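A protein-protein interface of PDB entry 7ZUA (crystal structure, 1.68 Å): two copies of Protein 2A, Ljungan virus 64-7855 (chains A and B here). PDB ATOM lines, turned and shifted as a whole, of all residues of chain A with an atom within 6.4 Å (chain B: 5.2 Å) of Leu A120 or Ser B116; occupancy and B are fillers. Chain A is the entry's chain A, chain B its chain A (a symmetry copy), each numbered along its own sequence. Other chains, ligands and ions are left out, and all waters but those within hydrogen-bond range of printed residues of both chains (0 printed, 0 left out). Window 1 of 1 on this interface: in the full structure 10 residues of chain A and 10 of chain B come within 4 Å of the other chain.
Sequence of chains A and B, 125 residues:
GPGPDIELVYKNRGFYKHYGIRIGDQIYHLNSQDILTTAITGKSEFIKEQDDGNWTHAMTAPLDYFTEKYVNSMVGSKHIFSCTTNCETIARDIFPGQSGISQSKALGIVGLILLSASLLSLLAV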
ATOM      1  N   ILE A  35      25.596  14.168  22.699  1.00  0.00           N
ATOM      2  CA  ILE A  35      25.714  15.608  22.633  1.00  0.00           C
ATOM      3  C   ILE A  35      26.645  16.145  23.717  1.00  0.00           C
ATOM      4  O   ILE A  35      27.432  17.042  23.437  1.00  0.00           O
ATOM      5  CB  ILE A  35      24.325  16.252  22.654  1.00  0.00           C
ATOM      6  CG1 ILE A  35      24.449  17.771  22.468  1.00  0.00           C
ATOM      7  CG2 ILE A  35      23.497  15.881  23.869  1.00  0.00           C
ATOM      8  CD1 ILE A  35      25.272  18.184  21.310  1.00  0.00           C
ATOM      9  N   TYR A  70      21.184  30.436  16.713  1.00  0.00           N
ATOM     10  CA  TYR A  70      22.192  29.548  17.236  1.00  0.00           C
ATOM     11  C   TYR A  70      23.575  30.092  16.910  1.00  0.00           C
ATOM     12  O   TYR A  70      24.570  29.562  17.400  1.00  0.00           O
ATOM     13  CB  TYR A  70      21.945  28.164  16.620  1.00  0.00           C
ATOM     14  CG  TYR A  70      20.588  27.578  16.920  1.00  0.00           C
ATOM     15  CD1 TYR A  70      19.995  27.704  18.175  1.00  0.00           C
ATOM     16  CD2 TYR A  70      19.918  26.841  15.965  1.00  0.00           C
ATOM     17  CE1 TYR A  70      18.766  27.127  18.451  1.00  0.00           C
ATOM     18  CE2 TYR A  70      18.693  26.255  16.228  1.00  0.00           C
ATOM     19  CZ  TYR A  70      18.125  26.380  17.479  1.00  0.00           C
ATOM     20  OH  TYR A  70      16.915  25.773  17.677  1.00  0.00           O
ATOM     21  N   LEU A 115      24.637  21.589  16.779  1.00  0.00           N
ATOM     22  CA  LEU A 115      25.002  21.452  18.171  1.00  0.00           C
ATOM     23  C   LEU A 115      23.955  22.079  19.084  1.00  0.00           C
ATOM     24  O   LEU A 115      23.577  21.533  20.119  1.00  0.00           O
ATOM     25  CB  LEU A 115      26.363  22.135  18.412  1.00  0.00           C
ATOM     26  CG  LEU A 115      27.622  21.306  18.145  1.00  0.00           C
ATOM     27  CD1 LEU A 115      28.862  22.086  18.562  1.00  0.00           C
ATOM     28  CD2 LEU A 115      27.589  19.966  18.869  1.00  0.00           C
ATOM     29  N   SER A 116      23.518  23.296  18.720  1.00  0.00           N
ATOM     30  CA  SER A 116      22.580  24.014  19.572  1.00  0.00           C
ATOM     31  C   SER A 116      21.247  23.277  19.656  1.00  0.00           C
ATOM     32  O   SER A 116      20.642  23.160  20.706  1.00  0.00           O
ATOM     33  CB  SER A 116      22.409  25.434  19.034  1.00  0.00           C
ATOM     34  OG  SER A 116      23.591  26.184  19.151  1.00  0.00           O
ATOM     35  N   ALA A 117      20.725  22.856  18.493  1.00  0.00           N
ATOM     36  CA  ALA A 117      19.469  22.137  18.470  1.00  0.00           C
ATOM     37  C   ALA A 117      19.592  20.845  19.305  1.00  0.00           C
ATOM     38  O   ALA A 117      18.684  20.537  20.073  1.00  0.00           O
ATOM     39  CB  ALA A 117      19.080  21.881  17.029  1.00  0.00           C
ATOM     40  N   SER A 118      20.717  20.098  19.173  1.00  0.00           N
ATOM     41  CA  SER A 118      20.860  18.856  19.938  1.00  0.00           C
ATOM     42  C   SER A 118      20.928  19.124  21.436  1.00  0.00           C
ATOM     43  O   SER A 118      20.319  18.415  22.258  1.00  0.00           O
ATOM     44  CB  SER A 118      22.047  18.045  19.496  1.00  0.00           C
ATOM     45  OG  SER A 118      21.804  17.469  18.240  1.00  0.00           O
ATOM     46  N   LEU A 119      21.669  20.176  21.816  1.00  0.00           N
ATOM     47  CA  LEU A 119      21.764  20.547  23.229  1.00  0.00           C
ATOM     48  C   LEU A 119      20.408  20.912  23.798  1.00  0.00           C
ATOM     49  O   LEU A 119      20.041  20.489  24.892  1.00  0.00           O
ATOM     50  CB  LEU A 119      22.697  21.748  23.417  1.00  0.00           C
ATOM     51  CG  LEU A 119      24.145  21.479  23.756  1.00  0.00           C
ATOM     52  CD1 LEU A 119      24.899  22.796  23.922  1.00  0.00           C
ATOM     53  CD2 LEU A 119      24.233  20.638  25.019  1.00  0.00           C
ATOM     54  N   LEU A 120      19.628  21.765  23.084  1.00  0.00           N
ATOM     55  CA  LEU A 120      18.331  22.136  23.582  1.00  0.00           C
ATOM     56  C   LEU A 120      17.387  20.932  23.614  1.00  0.00           C
ATOM     57  O   LEU A 120      16.462  20.942  24.402  1.00  0.00           O
ATOM     58  CB  LEU A 120      17.812  23.293  22.705  1.00  0.00           C
ATOM     59  CG  LEU A 120      18.623  24.578  22.856  1.00  0.00           C
ATOM     60  CD1 LEU A 120      18.079  25.651  21.918  1.00  0.00           C
ATOM     61  CD2 LEU A 120      18.654  25.092  24.290  1.00  0.00           C
ATOM     62  N   SER A 121      17.622  19.885  22.789  1.00  0.00           N
ATOM     63  CA  SER A 121      16.739  18.726  22.778  1.00  0.00           C
ATOM     64  C   SER A 121      16.765  17.959  24.103  1.00  0.00           C
ATOM     65  O   SER A 121      15.882  17.120  24.318  1.00  0.00           O
ATOM     66  CB  SER A 121      17.028  17.794  21.638  1.00  0.00           C
ATOM     67  OG  SER A 121      18.167  16.971  21.888  1.00  0.00           O
ATOM     68  N   LEU A 122      17.789  18.188  24.943  1.00  0.00           N
ATOM     69  CA  LEU A 122      17.843  17.595  26.284  1.00  0.00           C
ATOM     70  C   LEU A 122      16.605  17.982  27.084  1.00  0.00           C
ATOM     71  O   LEU A 122      16.162  17.236  27.965  1.00  0.00           O
ATOM     72  CB  LEU A 122      19.120  18.043  27.020  1.00  0.00           C
ATOM     73  CG  LEU A 122      20.438  17.501  26.475  1.00  0.00           C
ATOM     74  CD1 LEU A 122      21.616  18.085  27.245  1.00  0.00           C
ATOM     75  CD2 LEU A 122      20.468  15.978  26.553  1.00  0.00           C
ATOM     76  N   LEU A 123      16.010  19.146  26.778  1.00  0.00           N
ATOM     77  CA  LEU A 123      14.856  19.621  27.500  1.00  0.00           C
ATOM     78  C   LEU A 123      13.580  18.906  27.040  1.00  0.00           C
ATOM     79  O   LEU A 123      12.580  18.905  27.753  1.00  0.00           O
ATOM     80  CB  LEU A 123      14.768  21.138  27.278  1.00  0.00           C
ATOM     81  CG  LEU A 123      15.983  21.955  27.727  1.00  0.00           C
ATOM     82  CD1 LEU A 123      15.703  23.455  27.622  1.00  0.00           C
ATOM     83  CD2 LEU A 123      16.359  21.626  29.162  1.00  0.00           C
ATOM     84  N   ALA A 124      13.599  18.306  25.842  1.00  0.00           N
ATOM     85  CA  ALA A 124      12.386  17.774  25.233  1.00  0.00           C
ATOM     86  C   ALA A 124      12.224  16.275  25.483  1.00  0.00           C
ATOM     87  O   ALA A 124      11.246  15.683  25.027  1.00  0.00           O
ATOM     88  CB  ALA A 124      12.368  18.080  23.754  1.00  0.00           C
ATOM     89  N   TYR B  70      13.673  30.377  22.659  1.00  0.00           N
ATOM     90  CA  TYR B  70      13.884  29.360  23.658  1.00  0.00           C
ATOM     91  C   TYR B  70      12.552  28.736  24.047  1.00  0.00           C
ATOM     92  O   TYR B  70      12.531  27.745  24.773  1.00  0.00           O
ATOM     93  CB  TYR B  70      14.590  30.027  24.846  1.00  0.00           C
ATOM     94  CG  TYR B  70      15.920  30.655  24.513  1.00  0.00           C
ATOM     95  CD1 TYR B  70      16.823  30.044  23.646  1.00  0.00           C
ATOM     96  CD2 TYR B  70      16.306  31.836  25.114  1.00  0.00           C
ATOM     97  CE1 TYR B  70      18.060  30.610  23.378  1.00  0.00           C
ATOM     98  CE2 TYR B  70      17.539  32.410  24.860  1.00  0.00           C
ATOM     99  CZ  TYR B  70      18.425  31.787  24.006  1.00  0.00           C
ATOM    100  OH  TYR B  70      19.629  32.403  23.802  1.00  0.00           O
ATOM    101  N   GLY B 111      11.665  30.413  32.779  1.00  0.00           N
ATOM    102  CA  GLY B 111      12.509  29.266  33.078  1.00  0.00           C
ATOM    103  C   GLY B 111      13.178  28.697  31.825  1.00  0.00           C
ATOM    104  O   GLY B 111      14.362  28.366  31.837  1.00  0.00           O
ATOM    105  N   LEU B 112      12.418  28.594  30.726  1.00  0.00           N
ATOM    106  CA  LEU B 112      12.969  28.012  29.500  1.00  0.00           C
ATOM    107  C   LEU B 112      14.032  28.939  28.920  1.00  0.00           C
ATOM    108  O   LEU B 112      14.987  28.461  28.327  1.00  0.00           O
ATOM    109  CB  LEU B 112      11.864  27.815  28.456  1.00  0.00           C
ATOM    110  CG  LEU B 112      10.926  26.619  28.617  1.00  0.00           C
ATOM    111  CD1 LEU B 112      10.229  26.352  27.290  1.00  0.00           C
ATOM    112  CD2 LEU B 112      11.674  25.376  29.085  1.00  0.00           C
ATOM    113  N   ILE B 113      13.827  30.255  29.056  1.00  0.00           N
ATOM    114  CA  ILE B 113      14.813  31.211  28.562  1.00  0.00           C
ATOM    115  C   ILE B 113      16.116  30.994  29.318  1.00  0.00           C
ATOM    116  O   ILE B 113      17.171  30.886  28.700  1.00  0.00           O
ATOM    117  CB  ILE B 113      14.324  32.662  28.686  1.00  0.00           C
ATOM    118  CG1 ILE B 113      13.215  32.960  27.680  1.00  0.00           C
ATOM    119  CG2 ILE B 113      15.504  33.617  28.526  1.00  0.00           C
ATOM    120  CD1 ILE B 113      12.335  34.098  28.066  1.00  0.00           C
ATOM    121  N   LEU B 114      16.030  30.934  30.650  1.00  0.00           N
ATOM    122  CA  LEU B 114      17.224  30.827  31.478  1.00  0.00           C
ATOM    123  C   LEU B 114      17.929  29.484  31.281  1.00  0.00           C
ATOM    124  O   LEU B 114      19.157  29.433  31.132  1.00  0.00           O
ATOM    125  CB  LEU B 114      16.828  31.085  32.942  1.00  0.00           C
ATOM    126  CG  LEU B 114      16.234  32.462  33.255  1.00  0.00           C
ATOM    127  CD1 LEU B 114      15.992  32.573  34.744  1.00  0.00           C
ATOM    128  CD2 LEU B 114      17.122  33.609  32.772  1.00  0.00           C
ATOM    129  N   LEU B 115      17.166  28.374  31.260  1.00  0.00           N
ATOM    130  CA  LEU B 115      17.727  27.063  31.025  1.00  0.00           C
ATOM    131  C   LEU B 115      18.419  26.991  29.669  1.00  0.00           C
ATOM    132  O   LEU B 115      19.505  26.433  29.516  1.00  0.00           O
ATOM    133  CB  LEU B 115      16.605  26.008  31.082  1.00  0.00           C
ATOM    134  CG  LEU B 115      16.234  25.449  32.457  1.00  0.00           C
ATOM    135  CD1 LEU B 115      15.212  24.330  32.311  1.00  0.00           C
ATOM    136  CD2 LEU B 115      17.454  24.936  33.213  1.00  0.00           C
ATOM    137  N   SER B 116      17.739  27.519  28.639  1.00  0.00           N
ATOM    138  CA  SER B 116      18.278  27.425  27.289  1.00  0.00           C
ATOM    139  C   SER B 116      19.580  28.210  27.166  1.00  0.00           C
ATOM    140  O   SER B 116      20.541  27.771  26.560  1.00  0.00           O
ATOM    141  CB  SER B 116      17.224  27.917  26.298  1.00  0.00           C
ATOM    142  OG  SER B 116      16.105  27.070  26.260  1.00  0.00           O
ATOM    143  N   ALA B 117      19.576  29.453  27.672  1.00  0.00           N
ATOM    144  CA  ALA B 117      20.767  30.273  27.615  1.00  0.00           C
ATOM    145  C   ALA B 117      21.918  29.575  28.369  1.00  0.00           C
ATOM    146  O   ALA B 117      23.039  29.551  27.867  1.00  0.00           O
ATOM    147  CB  ALA B 117      20.441  31.646  28.162  1.00  0.00           C
ATOM    148  N   SER B 118      21.645  28.992  29.563  1.00  0.00           N
ATOM    149  CA  SER B 118      22.718  28.336  30.316  1.00  0.00           C
ATOM    150  C   SER B 118      23.258  27.117  29.576  1.00  0.00           C
ATOM    151  O   SER B 118      24.476  26.874  29.515  1.00  0.00           O
ATOM    152  CB  SER B 118      22.291  27.957  31.707  1.00  0.00           C
ATOM    153  OG  SER B 118      22.170  29.102  32.509  1.00  0.00           O
ATOM    154  N   LEU B 119      22.345  26.333  28.982  1.00  0.00           N
ATOM    155  CA  LEU B 119      22.762  25.163  28.208  1.00  0.00           C
ATOM    156  C   LEU B 119      23.631  25.558  27.031  1.00  0.00           C
ATOM    157  O   LEU B 119      24.662  24.944  26.766  1.00  0.00           O
ATOM    158  CB  LEU B 119      21.545  24.404  27.666  1.00  0.00           C
ATOM    159  CG  LEU B 119      21.014  23.241  28.472  1.00  0.00           C
ATOM    160  CD1 LEU B 119      19.822  22.609  27.758  1.00  0.00           C
ATOM    161  CD2 LEU B 119      22.118  22.220  28.695  1.00  0.00           C
ATOM    162  N   LEU B 120      23.208  26.583  26.246  1.00  0.00           N
ATOM    163  CA  LEU B 120      24.003  26.997  25.121  1.00  0.00           C
ATOM    164  C   LEU B 120      25.338  27.590  25.577  1.00  0.00           C
ATOM    165  O   LEU B 120      26.280  27.553  24.810  1.00  0.00           O
ATOM    166  CB  LEU B 120      23.153  27.979  24.289  1.00  0.00           C
ATOM    167  CG  LEU B 120      21.939  27.323  23.635  1.00  0.00           C
ATOM    168  CD1 LEU B 120      21.126  28.370  22.880  1.00  0.00           C
ATOM    169  CD2 LEU B 120      22.316  26.173  22.709  1.00  0.00           C
ATOM    170  N   SER B 121      25.439  28.111  26.821  1.00  0.00           N
ATOM    171  CA  SER B 121      26.689  28.699  27.289  1.00  0.00           C
ATOM    172  C   SER B 121      27.814  27.667  27.401  1.00  0.00           C
ATOM    173  O   SER B 121      28.975  28.071  27.533  1.00  0.00           O
ATOM    174  CB  SER B 121      26.529  29.429  28.589  1.00  0.00           C
ATOM    175  OG  SER B 121      26.485  28.541  29.706  1.00  0.00           O
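The backbone carbonyl oxygen of Leu B112 sits at hydrogen-bond distance from the side-chain hydroxyl of Ser B116.
Among the printed residues, merely in contact across the chains: Leu A119 with Leu B119 (3.6 Å), Leu A120 with Ser B116 (3.7 Å), Ser A116 with Leu B120 (3.7 Å), Leu A123 with Leu B119 (3.9 Å) and Leu A123 with Ser B116 (3.9 Å).
Of chain B, only Ser B116 (3.7 Å) comes within 4 Å of Leu A120. Printed residues of chain B within 4 Å of Leu A123: Ser B116 (3.9 Å) and Leu B119 (3.9 Å). Ser B116 touches just these residues of chain A: Leu A120 and Leu A123. Ala B117 touches none of the printed residues of chain A. Printed residues of chain A within 4 Å of Leu B119: Leu A119 and Leu A123. The nearest residue of chain B that does not touch Leu A120 is Leu B120 (4.02 Å). The nearest printed residue of chain A that does not touch Ser B116 is Leu A119 (7.1 Å).
Of the 12 printed residues of chain A, 4 touch a printed residue of chain B. Hydrophobic or aromatic side chains of chain A that line the printed part of chain B: Leu A119, Leu A120 and Leu A123. Among the printed residues, 5 pairs touch across the chains.
Ser A116 touches Leu B120, and with the chains exchanged Leu A120 touches Ser B116. Leu A119 touches its own counterpart, Leu B119. 8 positions are printed for both chains.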
